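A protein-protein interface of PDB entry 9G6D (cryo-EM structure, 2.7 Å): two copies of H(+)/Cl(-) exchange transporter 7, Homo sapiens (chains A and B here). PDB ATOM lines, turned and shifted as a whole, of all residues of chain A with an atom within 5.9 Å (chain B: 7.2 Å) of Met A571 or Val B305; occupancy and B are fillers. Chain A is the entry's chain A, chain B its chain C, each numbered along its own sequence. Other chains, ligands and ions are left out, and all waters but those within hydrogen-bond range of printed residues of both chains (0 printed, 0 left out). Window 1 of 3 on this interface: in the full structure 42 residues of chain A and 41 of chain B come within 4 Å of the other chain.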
ATOM      1  N   VAL A 305     -30.082 -25.644   3.494  1.00  0.00           N
ATOM      2  CA  VAL A 305     -28.900 -25.050   2.878  1.00  0.00           C
ATOM      3  C   VAL A 305     -27.892 -24.643   3.943  1.00  0.00           C
ATOM      4  O   VAL A 305     -26.678 -24.781   3.753  1.00  0.00           O
ATOM      5  CB  VAL A 305     -29.297 -23.861   1.985  1.00  0.00           C
ATOM      6  CG1 VAL A 305     -28.093 -23.363   1.205  1.00  0.00           C
ATOM      7  CG2 VAL A 305     -30.417 -24.260   1.043  1.00  0.00           C
ATOM      8  N   LEU A 309     -23.904 -25.645   4.235  1.00  0.00           N
ATOM      9  CA  LEU A 309     -22.829 -24.686   4.457  1.00  0.00           C
ATOM     10  C   LEU A 309     -22.040 -25.026   5.712  1.00  0.00           C
ATOM     11  O   LEU A 309     -20.809 -24.918   5.728  1.00  0.00           O
ATOM     12  CB  LEU A 309     -23.397 -23.270   4.546  1.00  0.00           C
ATOM     13  CG  LEU A 309     -23.287 -22.411   3.286  1.00  0.00           C
ATOM     14  CD1 LEU A 309     -21.838 -22.040   3.026  1.00  0.00           C
ATOM     15  CD2 LEU A 309     -23.882 -23.127   2.087  1.00  0.00           C
ATOM     16  N   LEU A 566     -24.239 -19.229   9.998  1.00  0.00           N
ATOM     17  CA  LEU A 566     -25.330 -18.696  10.806  1.00  0.00           C
ATOM     18  C   LEU A 566     -26.246 -17.809   9.971  1.00  0.00           C
ATOM     19  O   LEU A 566     -27.472 -17.916  10.065  1.00  0.00           O
ATOM     20  CB  LEU A 566     -24.759 -17.928  12.001  1.00  0.00           C
ATOM     21  CG  LEU A 566     -25.551 -17.726  13.301  1.00  0.00           C
ATOM     22  CD1 LEU A 566     -24.786 -16.815  14.243  1.00  0.00           C
ATOM     23  CD2 LEU A 566     -26.951 -17.184  13.090  1.00  0.00           C
ATOM     24  N   THR A 567     -25.669 -16.940   9.134  1.00  0.00           N
ATOM     25  CA  THR A 567     -26.494 -16.007   8.372  1.00  0.00           C
ATOM     26  C   THR A 567     -27.409 -16.741   7.401  1.00  0.00           C
ATOM     27  O   THR A 567     -28.579 -16.374   7.250  1.00  0.00           O
ATOM     28  CB  THR A 567     -25.620 -14.992   7.630  1.00  0.00           C
ATOM     29  OG1 THR A 567     -26.445 -14.174   6.793  1.00  0.00           O
ATOM     30  CG2 THR A 567     -24.576 -15.683   6.782  1.00  0.00           C
ATOM     31  N   VAL A 568     -26.904 -17.791   6.753  1.00  0.00           N
ATOM     32  CA  VAL A 568     -27.721 -18.557   5.816  1.00  0.00           C
ATOM     33  C   VAL A 568     -28.918 -19.164   6.535  1.00  0.00           C
ATOM     34  O   VAL A 568     -30.019 -19.252   5.980  1.00  0.00           O
ATOM     35  CB  VAL A 568     -26.866 -19.633   5.122  1.00  0.00           C
ATOM     36  CG1 VAL A 568     -27.719 -20.480   4.194  1.00  0.00           C
ATOM     37  CG2 VAL A 568     -25.723 -18.987   4.362  1.00  0.00           C
ATOM     38  N   ILE A 569     -28.721 -19.587   7.785  1.00  0.00           N
ATOM     39  CA  ILE A 569     -29.819 -20.137   8.572  1.00  0.00           C
ATOM     40  C   ILE A 569     -30.895 -19.082   8.805  1.00  0.00           C
ATOM     41  O   ILE A 569     -32.094 -19.365   8.689  1.00  0.00           O
ATOM     42  CB  ILE A 569     -29.284 -20.710   9.897  1.00  0.00           C
ATOM     43  CG1 ILE A 569     -28.476 -21.980   9.632  1.00  0.00           C
ATOM     44  CG2 ILE A 569     -30.422 -20.995  10.859  1.00  0.00           C
ATOM     45  CD1 ILE A 569     -27.507 -22.329  10.734  1.00  0.00           C
ATOM     46  N   MET A 570     -30.489 -17.852   9.130  1.00  0.00           N
ATOM     47  CA  MET A 570     -31.464 -16.800   9.407  1.00  0.00           C
ATOM     48  C   MET A 570     -32.313 -16.477   8.182  1.00  0.00           C
ATOM     49  O   MET A 570     -33.535 -16.338   8.286  1.00  0.00           O
ATOM     50  CB  MET A 570     -30.765 -15.544   9.926  1.00  0.00           C
ATOM     51  CG  MET A 570     -29.628 -15.815  10.886  1.00  0.00           C
ATOM     52  SD  MET A 570     -30.227 -16.049  12.571  1.00  0.00           S
ATOM     53  CE  MET A 570     -31.576 -14.873  12.626  1.00  0.00           C
ATOM     54  N   MET A 571     -31.685 -16.351   7.008  1.00  0.00           N
ATOM     55  CA  MET A 571     -32.472 -16.103   5.803  1.00  0.00           C
ATOM     56  C   MET A 571     -33.414 -17.265   5.520  1.00  0.00           C
ATOM     57  O   MET A 571     -34.559 -17.057   5.105  1.00  0.00           O
ATOM     58  CB  MET A 571     -31.566 -15.845   4.599  1.00  0.00           C
ATOM     59  CG  MET A 571     -30.190 -15.319   4.932  1.00  0.00           C
ATOM     60  SD  MET A 571     -29.160 -15.115   3.468  1.00  0.00           S
ATOM     61  CE  MET A 571     -30.260 -14.170   2.419  1.00  0.00           C
ATOM     62  N   GLU A 572     -32.949 -18.495   5.736  1.00  0.00           N
ATOM     63  CA  GLU A 572     -33.829 -19.647   5.575  1.00  0.00           C
ATOM     64  C   GLU A 572     -34.906 -19.675   6.651  1.00  0.00           C
ATOM     65  O   GLU A 572     -36.057 -20.034   6.375  1.00  0.00           O
ATOM     66  CB  GLU A 572     -33.012 -20.937   5.598  1.00  0.00           C
ATOM     67  CG  GLU A 572     -32.395 -21.288   4.260  1.00  0.00           C
ATOM     68  CD  GLU A 572     -31.564 -22.550   4.315  1.00  0.00           C
ATOM     69  OE1 GLU A 572     -30.444 -22.503   4.864  1.00  0.00           O
ATOM     70  OE2 GLU A 572     -32.034 -23.589   3.810  1.00  0.00           O
ATOM     71  N   ALA A 573     -34.555 -19.303   7.883  1.00  0.00           N
ATOM     72  CA  ALA A 573     -35.531 -19.325   8.968  1.00  0.00           C
ATOM     73  C   ALA A 573     -36.601 -18.257   8.770  1.00  0.00           C
ATOM     74  O   ALA A 573     -37.799 -18.538   8.884  1.00  0.00           O
ATOM     75  CB  ALA A 573     -34.826 -19.142  10.311  1.00  0.00           C
ATOM     76  N   THR A 574     -36.188 -17.024   8.474  1.00  0.00           N
ATOM     77  CA  THR A 574     -37.147 -15.951   8.249  1.00  0.00           C
ATOM     78  C   THR A 574     -37.773 -15.999   6.862  1.00  0.00           C
ATOM     79  O   THR A 574     -38.815 -15.369   6.650  1.00  0.00           O
ATOM     80  CB  THR A 574     -36.486 -14.587   8.462  1.00  0.00           C
ATOM     81  OG1 THR A 574     -35.647 -14.276   7.345  1.00  0.00           O
ATOM     82  CG2 THR A 574     -35.665 -14.581   9.740  1.00  0.00           C
ATOM     83  N   SER A 575     -37.169 -16.733   5.925  1.00  0.00           N
ATOM     84  CA  SER A 575     -37.688 -16.867   4.564  1.00  0.00           C
ATOM     85  C   SER A 575     -37.891 -15.503   3.911  1.00  0.00           C
ATOM     86  O   SER A 575     -38.912 -15.240   3.271  1.00  0.00           O
ATOM     87  CB  SER A 575     -38.983 -17.680   4.549  1.00  0.00           C
ATOM     88  OG  SER A 575     -38.711 -19.066   4.449  1.00  0.00           O
ATOM     89  N   ASN A 576     -36.908 -14.620   4.079  1.00  0.00           N
ATOM     90  CA  ASN A 576     -36.963 -13.270   3.519  1.00  0.00           C
ATOM     91  C   ASN A 576     -35.544 -12.867   3.133  1.00  0.00           C
ATOM     92  O   ASN A 576     -34.724 -12.559   4.002  1.00  0.00           O
ATOM     93  CB  ASN A 576     -37.571 -12.287   4.511  1.00  0.00           C
ATOM     94  CG  ASN A 576     -37.829 -10.929   3.900  1.00  0.00           C
ATOM     95  OD1 ASN A 576     -36.983 -10.038   3.963  1.00  0.00           O
ATOM     96  ND2 ASN A 576     -39.001 -10.761   3.304  1.00  0.00           N
ATOM     97  N   VAL A 577     -35.257 -12.876   1.829  1.00  0.00           N
ATOM     98  CA  VAL A 577     -33.926 -12.518   1.356  1.00  0.00           C
ATOM     99  C   VAL A 577     -33.635 -11.036   1.539  1.00  0.00           C
ATOM    100  O   VAL A 577     -32.465 -10.645   1.619  1.00  0.00           O
ATOM    101  CB  VAL A 577     -33.746 -12.925  -0.118  1.00  0.00           C
ATOM    102  CG1 VAL A 577     -33.783 -14.437  -0.257  1.00  0.00           C
ATOM    103  CG2 VAL A 577     -34.821 -12.285  -0.978  1.00  0.00           C
ATOM    104  N   TYR A 579     -34.135  -9.314   4.164  1.00  0.00           N
ATOM    105  CA  TYR A 579     -33.556  -9.161   5.491  1.00  0.00           C
ATOM    106  C   TYR A 579     -32.193  -9.814   5.630  1.00  0.00           C
ATOM    107  O   TYR A 579     -31.585  -9.709   6.698  1.00  0.00           O
ATOM    108  CB  TYR A 579     -34.498  -9.727   6.551  1.00  0.00           C
ATOM    109  CG  TYR A 579     -35.518  -8.730   7.019  1.00  0.00           C
ATOM    110  CD1 TYR A 579     -36.872  -8.991   6.912  1.00  0.00           C
ATOM    111  CD2 TYR A 579     -35.123  -7.523   7.576  1.00  0.00           C
ATOM    112  CE1 TYR A 579     -37.806  -8.078   7.339  1.00  0.00           C
ATOM    113  CE2 TYR A 579     -36.047  -6.604   8.010  1.00  0.00           C
ATOM    114  CZ  TYR A 579     -37.387  -6.887   7.888  1.00  0.00           C
ATOM    115  OH  TYR A 579     -38.309  -5.968   8.321  1.00  0.00           O
ATOM    116  N   GLY A 580     -31.703 -10.490   4.593  1.00  0.00           N
ATOM    117  CA  GLY A 580     -30.368 -11.057   4.670  1.00  0.00           C
ATOM    118  C   GLY A 580     -29.296  -9.994   4.813  1.00  0.00           C
ATOM    119  O   GLY A 580     -28.328 -10.173   5.554  1.00  0.00           O
ATOM    120  N   PHE A 581     -29.450  -8.880   4.097  1.00  0.00           N
ATOM    121  CA  PHE A 581     -28.455  -7.813   4.166  1.00  0.00           C
ATOM    122  C   PHE A 581     -28.339  -7.193   5.554  1.00  0.00           C
ATOM    123  O   PHE A 581     -27.210  -7.109   6.069  1.00  0.00           O
ATOM    124  CB  PHE A 581     -28.758  -6.757   3.097  1.00  0.00           C
ATOM    125  CG  PHE A 581     -27.706  -5.697   2.982  1.00  0.00           C
ATOM    126  CD1 PHE A 581     -26.405  -6.028   2.656  1.00  0.00           C
ATOM    127  CD2 PHE A 581     -28.019  -4.368   3.206  1.00  0.00           C
ATOM    128  CE1 PHE A 581     -25.435  -5.055   2.552  1.00  0.00           C
ATOM    129  CE2 PHE A 581     -27.053  -3.390   3.103  1.00  0.00           C
ATOM    130  CZ  PHE A 581     -25.759  -3.733   2.775  1.00  0.00           C
ATOM    131  N   ILE A 583     -29.207  -8.578   8.335  1.00  0.00           N
ATOM    132  CA  ILE A 583     -28.723  -9.687   9.152  1.00  0.00           C
ATOM    133  C   ILE A 583     -27.230  -9.886   8.939  1.00  0.00           C
ATOM    134  O   ILE A 583     -26.475 -10.119   9.890  1.00  0.00           O
ATOM    135  CB  ILE A 583     -29.523 -10.965   8.840  1.00  0.00           C
ATOM    136  CG1 ILE A 583     -30.853 -10.958   9.593  1.00  0.00           C
ATOM    137  CG2 ILE A 583     -28.729 -12.207   9.189  1.00  0.00           C
ATOM    138  CD1 ILE A 583     -31.821 -12.017   9.123  1.00  0.00           C
ATOM    139  N   VAL B 297     -25.700 -13.739 -10.433  1.00  0.00           N
ATOM    140  CA  VAL B 297     -26.757 -14.699 -10.125  1.00  0.00           C
ATOM    141  C   VAL B 297     -27.683 -14.143  -9.055  1.00  0.00           C
ATOM    142  O   VAL B 297     -28.909 -14.279  -9.138  1.00  0.00           O
ATOM    143  CB  VAL B 297     -26.153 -16.049  -9.696  1.00  0.00           C
ATOM    144  CG1 VAL B 297     -27.255 -17.042  -9.378  1.00  0.00           C
ATOM    145  CG2 VAL B 297     -25.242 -16.596 -10.774  1.00  0.00           C
ATOM    146  N   SER B 298     -27.110 -13.515  -8.026  1.00  0.00           N
ATOM    147  CA  SER B 298     -27.922 -12.949  -6.955  1.00  0.00           C
ATOM    148  C   SER B 298     -28.829 -11.840  -7.474  1.00  0.00           C
ATOM    149  O   SER B 298     -30.004 -11.768  -7.103  1.00  0.00           O
ATOM    150  CB  SER B 298     -27.019 -12.428  -5.841  1.00  0.00           C
ATOM    151  OG  SER B 298     -27.571 -11.272  -5.240  1.00  0.00           O
ATOM    152  N   GLY B 302     -32.480 -12.867  -7.268  1.00  0.00           N
ATOM    153  CA  GLY B 302     -32.702 -12.573  -5.864  1.00  0.00           C
ATOM    154  C   GLY B 302     -32.331 -13.721  -4.952  1.00  0.00           C
ATOM    155  O   GLY B 302     -33.015 -13.960  -3.949  1.00  0.00           O
ATOM    156  N   ALA B 303     -31.259 -14.440  -5.277  1.00  0.00           N
ATOM    157  CA  ALA B 303     -30.815 -15.608  -4.519  1.00  0.00           C
ATOM    158  C   ALA B 303     -29.339 -15.438  -4.188  1.00  0.00           C
ATOM    159  O   ALA B 303     -28.471 -16.015  -4.856  1.00  0.00           O
ATOM    160  CB  ALA B 303     -31.063 -16.899  -5.299  1.00  0.00           C
ATOM    161  N   PRO B 304     -29.019 -14.638  -3.168  1.00  0.00           N
ATOM    162  CA  PRO B 304     -27.602 -14.448  -2.811  1.00  0.00           C
ATOM    163  C   PRO B 304     -26.889 -15.735  -2.437  1.00  0.00           C
ATOM    164  O   PRO B 304     -25.705 -15.896  -2.757  1.00  0.00           O
ATOM    165  CB  PRO B 304     -27.668 -13.469  -1.629  1.00  0.00           C
ATOM    166  CG  PRO B 304     -29.069 -13.539  -1.132  1.00  0.00           C
ATOM    167  CD  PRO B 304     -29.921 -13.855  -2.311  1.00  0.00           C
ATOM    168  N   VAL B 305     -27.573 -16.657  -1.759  1.00  0.00           N
ATOM    169  CA  VAL B 305     -26.949 -17.931  -1.414  1.00  0.00           C
ATOM    170  C   VAL B 305     -26.757 -18.784  -2.660  1.00  0.00           C
ATOM    171  O   VAL B 305     -25.730 -19.456  -2.817  1.00  0.00           O
ATOM    172  CB  VAL B 305     -27.776 -18.665  -0.345  1.00  0.00           C
ATOM    173  CG1 VAL B 305     -27.051 -19.918   0.111  1.00  0.00           C
ATOM    174  CG2 VAL B 305     -28.047 -17.747   0.833  1.00  0.00           C
ATOM    175  N   GLY B 306     -27.738 -18.774  -3.564  1.00  0.00           N
ATOM    176  CA  GLY B 306     -27.593 -19.519  -4.804  1.00  0.00           C
ATOM    177  C   GLY B 306     -26.439 -19.019  -5.651  1.00  0.00           C
ATOM    178  O   GLY B 306     -25.769 -19.801  -6.328  1.00  0.00           O
ATOM    179  N   GLY B 307     -26.197 -17.708  -5.630  1.00  0.00           N
ATOM    180  CA  GLY B 307     -25.053 -17.170  -6.345  1.00  0.00           C
ATOM    181  C   GLY B 307     -23.735 -17.655  -5.777  1.00  0.00           C
ATOM    182  O   GLY B 307     -22.799 -17.954  -6.522  1.00  0.00           O
ATOM    183  N   VAL B 308     -23.642 -17.735  -4.449  1.00  0.00           N
ATOM    184  CA  VAL B 308     -22.428 -18.234  -3.811  1.00  0.00           C
ATOM    185  C   VAL B 308     -22.206 -19.696  -4.167  1.00  0.00           C
ATOM    186  O   VAL B 308     -21.075 -20.124  -4.432  1.00  0.00           O
ATOM    187  CB  VAL B 308     -22.507 -18.024  -2.290  1.00  0.00           C
ATOM    188  CG1 VAL B 308     -21.364 -18.739  -1.585  1.00  0.00           C
ATOM    189  CG2 VAL B 308     -22.498 -16.551  -1.980  1.00  0.00           C
ATOM    190  N   LEU B 309     -23.281 -20.486  -4.173  1.00  0.00           N
ATOM    191  CA  LEU B 309     -23.176 -21.875  -4.607  1.00  0.00           C
ATOM    192  C   LEU B 309     -22.725 -21.964  -6.058  1.00  0.00           C
ATOM    193  O   LEU B 309     -21.892 -22.807  -6.404  1.00  0.00           O
ATOM    194  CB  LEU B 309     -24.515 -22.588  -4.420  1.00  0.00           C
ATOM    195  CG  LEU B 309     -24.682 -23.446  -3.166  1.00  0.00           C
ATOM    196  CD1 LEU B 309     -23.781 -24.667  -3.238  1.00  0.00           C
ATOM    197  CD2 LEU B 309     -24.394 -22.642  -1.914  1.00  0.00           C
ATOM    198  N   PHE B 310     -23.255 -21.092  -6.919  1.00  0.00           N
ATOM    199  CA  PHE B 310     -22.861 -21.101  -8.324  1.00  0.00           C
ATOM    200  C   PHE B 310     -21.369 -20.844  -8.478  1.00  0.00           C
ATOM    201  O   PHE B 310     -20.697 -21.504  -9.277  1.00  0.00           O
ATOM    202  CB  PHE B 310     -23.675 -20.063  -9.097  1.00  0.00           C
ATOM    203  CG  PHE B 310     -23.390 -20.036 -10.573  1.00  0.00           C
ATOM    204  CD1 PHE B 310     -22.350 -19.274 -11.083  1.00  0.00           C
ATOM    205  CD2 PHE B 310     -24.158 -20.780 -11.451  1.00  0.00           C
ATOM    206  CE1 PHE B 310     -22.089 -19.252 -12.437  1.00  0.00           C
ATOM    207  CE2 PHE B 310     -23.899 -20.761 -12.806  1.00  0.00           C
ATOM    208  CZ  PHE B 310     -22.863 -19.996 -13.300  1.00  0.00           C
ATOM    209  N   SER B 311     -20.831 -19.887  -7.723  1.00  0.00           N
ATOM    210  CA  SER B 311     -19.399 -19.629  -7.784  1.00  0.00           C
ATOM    211  C   SER B 311     -18.595 -20.772  -7.182  1.00  0.00           C
ATOM    212  O   SER B 311     -17.441 -20.986  -7.566  1.00  0.00           O
ATOM    213  CB  SER B 311     -19.076 -18.317  -7.072  1.00  0.00           C
ATOM    214  OG  SER B 311     -19.044 -17.238  -7.988  1.00  0.00           O
ATOM    215  N   PHE B 328     -19.917 -13.968  -0.736  1.00  0.00           N
ATOM    216  CA  PHE B 328     -21.225 -13.761  -0.120  1.00  0.00           C
ATOM    217  C   PHE B 328     -21.510 -12.282   0.094  1.00  0.00           C
ATOM    218  O   PHE B 328     -22.646 -11.830  -0.084  1.00  0.00           O
ATOM    219  CB  PHE B 328     -21.309 -14.517   1.204  1.00  0.00           C
ATOM    220  CG  PHE B 328     -22.711 -14.710   1.700  1.00  0.00           C
ATOM    221  CD1 PHE B 328     -23.716 -15.111   0.840  1.00  0.00           C
ATOM    222  CD2 PHE B 328     -23.027 -14.481   3.025  1.00  0.00           C
ATOM    223  CE1 PHE B 328     -25.006 -15.286   1.291  1.00  0.00           C
ATOM    224  CE2 PHE B 328     -24.318 -14.652   3.480  1.00  0.00           C
ATOM    225  CZ  PHE B 328     -25.308 -15.056   2.613  1.00  0.00           C
ATOM    226  N   SER B 331     -22.459 -10.902  -3.233  1.00  0.00           N
ATOM    227  CA  SER B 331     -23.757 -11.408  -3.663  1.00  0.00           C
ATOM    228  C   SER B 331     -24.896 -10.694  -2.951  1.00  0.00           C
ATOM    229  O   SER B 331     -25.906 -10.346  -3.574  1.00  0.00           O
ATOM    230  CB  SER B 331     -23.837 -12.913  -3.419  1.00  0.00           C
ATOM    231  OG  SER B 331     -22.950 -13.612  -4.270  1.00  0.00           O
ATOM    232  N   MET B 332     -24.760 -10.470  -1.644  1.00  0.00           N
ATOM    233  CA  MET B 332     -25.842  -9.840  -0.899  1.00  0.00           C
ATOM    234  C   MET B 332     -25.893  -8.335  -1.122  1.00  0.00           C
ATOM    235  O   MET B 332     -26.976  -7.743  -1.071  1.00  0.00           O
ATOM    236  CB  MET B 332     -25.711 -10.141   0.592  1.00  0.00           C
ATOM    237  CG  MET B 332     -26.059 -11.572   0.941  1.00  0.00           C
ATOM    238  SD  MET B 332     -27.192 -11.665   2.326  1.00  0.00           S
ATOM    239  CE  MET B 332     -28.587 -10.818   1.594  1.00  0.00           C
ATOM    240  N   THR B 335     -27.884  -7.872  -4.568  1.00  0.00           N
ATOM    241  CA  THR B 335     -29.340  -7.957  -4.543  1.00  0.00           C
ATOM    242  C   THR B 335     -29.958  -6.814  -3.749  1.00  0.00           C
ATOM    243  O   THR B 335     -31.094  -6.415  -4.027  1.00  0.00           O
ATOM    244  CB  THR B 335     -29.788  -9.305  -3.976  1.00  0.00           C
ATOM    245  OG1 THR B 335     -31.214  -9.315  -3.836  1.00  0.00           O
ATOM    246  CG2 THR B 335     -29.152  -9.563  -2.625  1.00  0.00           C
ATOM    247  N   SER B 565     -26.940 -25.417  -7.532  1.00  0.00           N
ATOM    248  CA  SER B 565     -27.191 -23.981  -7.476  1.00  0.00           C
ATOM    249  C   SER B 565     -28.610 -23.643  -7.903  1.00  0.00           C
ATOM    250  O   SER B 565     -29.204 -22.691  -7.384  1.00  0.00           O
ATOM    251  CB  SER B 565     -26.179 -23.243  -8.349  1.00  0.00           C
ATOM    252  OG  SER B 565     -25.874 -23.994  -9.509  1.00  0.00           O
ATOM    253  N   VAL B 568     -31.067 -24.255  -4.790  1.00  0.00           N
ATOM    254  CA  VAL B 568     -31.050 -23.187  -3.796  1.00  0.00           C
ATOM    255  C   VAL B 568     -31.754 -21.946  -4.325  1.00  0.00           C
ATOM    256  O   VAL B 568     -32.375 -21.201  -3.558  1.00  0.00           O
ATOM    257  CB  VAL B 568     -29.604 -22.877  -3.372  1.00  0.00           C
ATOM    258  CG1 VAL B 568     -29.590 -22.114  -2.060  1.00  0.00           C
ATOM    259  CG2 VAL B 568     -28.803 -24.159  -3.251  1.00  0.00           C
ATOM    260  N   ILE B 569     -31.666 -21.700  -5.633  1.00  0.00           N
ATOM    261  CA  ILE B 569     -32.292 -20.518  -6.219  1.00  0.00           C
ATOM    262  C   ILE B 569     -33.808 -20.581  -6.070  1.00  0.00           C
ATOM    263  O   ILE B 569     -34.453 -19.579  -5.739  1.00  0.00           O
ATOM    264  CB  ILE B 569     -31.862 -20.368  -7.689  1.00  0.00           C
ATOM    265  CG1 ILE B 569     -30.474 -19.732  -7.768  1.00  0.00           C
ATOM    266  CG2 ILE B 569     -32.866 -19.536  -8.466  1.00  0.00           C
ATOM    267  CD1 ILE B 569     -29.767 -19.964  -9.081  1.00  0.00           C
ATOM    268  N   GLU B 572     -34.922 -19.775  -2.476  1.00  0.00           N
ATOM    269  CA  GLU B 572     -34.769 -18.347  -2.229  1.00  0.00           C
ATOM    270  C   GLU B 572     -35.763 -17.532  -3.043  1.00  0.00           C
ATOM    271  O   GLU B 572     -36.235 -16.489  -2.578  1.00  0.00           O
ATOM    272  CB  GLU B 572     -33.337 -17.914  -2.531  1.00  0.00           C
ATOM    273  CG  GLU B 572     -32.359 -18.262  -1.428  1.00  0.00           C
ATOM    274  CD  GLU B 572     -30.935 -17.879  -1.764  1.00  0.00           C
ATOM    275  OE1 GLU B 572     -30.310 -18.574  -2.591  1.00  0.00           O
ATOM    276  OE2 GLU B 572     -30.442 -16.879  -1.201  1.00  0.00           O
ATOM    277  N   SER B 575     -39.133 -18.536  -1.375  1.00  0.00           N
ATOM    278  CA  SER B 575     -39.136 -18.221   0.055  1.00  0.00           C
ATOM    279  C   SER B 575     -39.946 -19.245   0.847  1.00  0.00           C
ATOM    280  O   SER B 575     -40.700 -18.899   1.757  1.00  0.00           O
ATOM    281  CB  SER B 575     -39.652 -16.803   0.310  1.00  0.00           C
ATOM    282  OG  SER B 575     -41.063 -16.746   0.208  1.00  0.00           O
ATOM    283  N   VAL B 577     -39.150 -23.109   2.479  1.00  0.00           N
ATOM    284  CA  VAL B 577     -38.235 -24.228   2.690  1.00  0.00           C
ATOM    285  C   VAL B 577     -38.943 -25.555   2.441  1.00  0.00           C
ATOM    286  O   VAL B 577     -38.356 -26.493   1.887  1.00  0.00           O
ATOM    287  CB  VAL B 577     -37.626 -24.153   4.102  1.00  0.00           C
ATOM    288  CG1 VAL B 577     -37.236 -25.533   4.605  1.00  0.00           C
ATOM    289  CG2 VAL B 577     -36.421 -23.227   4.107  1.00  0.00           C
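The backbone carbonyl oxygen of Gly A580 lies close to the side-chain sulfur of Met B332 (3.7 Å). OG of Ser A575 sits at hydrogen-bond distance from O of Ser B575, 3.4 Å away.
OE1 of Glu B572 is in hydrogen-bond range of N of Gly B306 (2.8 Å). The side-chain hydroxyl of Ser A575 is in hydrogen-bond range of the backbone carbonyl oxygen of Glu A572, 3.4 Å away. The backbone NH (N) of Val B305 sits at hydrogen-bond distance from the side-chain carboxylate (OE2) of Glu B572, at 2.9 Å. OE2 of Glu A572 lies within hydrogen-bond range of N of Val A305 (2.9 Å).
CG1 of Val A305 touches CG1 of Val B305, 3.8 Å away. CG1 of Val A305 touches CG1 of Val B568, at 3.8 Å. Phe B328 touches Thr A567. Pro B304 touches Met A571. Met A571 touches Val B305. Val B577 touches Glu A572 (CG2 to O, 3.9 Å). Gly B302 touches Val A577. O of Val A577 touches CE of Met B332, 3.9 Å away. CG1 of Val A577 touches O of Glu B572, 3.95 Å away. CE of Met B332 touches N of Phe A581, at 3.3 Å.
Of chain B, only Pro B304 (3.8 Å), Val B305 (3.9 Å), Phe B328 (3.9 Å) and Met B332 (3.8 Å) come within 4 Å of Met A571. Val B305 touches just these residues of chain A: Val A305 and Met A571. Printed residues of chain B within 4 Å of Ser A575: Ser B575 (3.4 Å). Of the printed residues of chain B, Thr A567 touches Phe B328 (3.5 Å). Of the printed residues of chain A, Met B332 touches Met A571 (3.8 Å), Val A577 (3.9 Å), Gly A580 (3.4 Å) and Phe A581 (3.3 Å). Tyr A579 touches none of the printed residues of chain B. Ala B303 touches none of the printed residues of chain A. The nearest residue of chain A that does not touch Val B305 is Val A568 (4.2 Å).
Val A305 touches its own counterpart, Val B305. Val A305 touches Val B568, but with the chains exchanged Val A568 does not touch Val B305 (4.2 Å). Glu A572 touches Val B577, and with the chains exchanged Val A577 touches Glu B572. Ser A575 touches its own counterpart, Ser B575. Of the 14 pairs that touch across the chains among the printed residues, 4 have their exchanged pair printed and touching as well.
Printed residues of chain A that touch a printed residue of chain B: Val A305, Thr A567, Met A571, Glu A572, Ser A575, Val A577, Gly A580 and Phe A581. Hydrophobic or aromatic side chains of chain A that line the printed part of chain B: Val A305, Met A571 and Val A577. Of the 22 printed residues of chain B, 9 touch a printed residue of chain A. Printed residues of chain B that touch a printed residue of chain A: Gly B302, Pro B304, Val B305, Phe B328, Met B332, Val B568, Glu B572, Ser B575 and Val B577. Hydrophobic or aromatic side chains of chain B that line the printed part of chain A: Pro B304, Val B305, Phe B328, Met B332, Val B568 and Val B577. Among the printed residues, no Asp or Glu carboxylate lies within 4 Å of a Lys or Arg side-chain nitrogen of the other chain.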
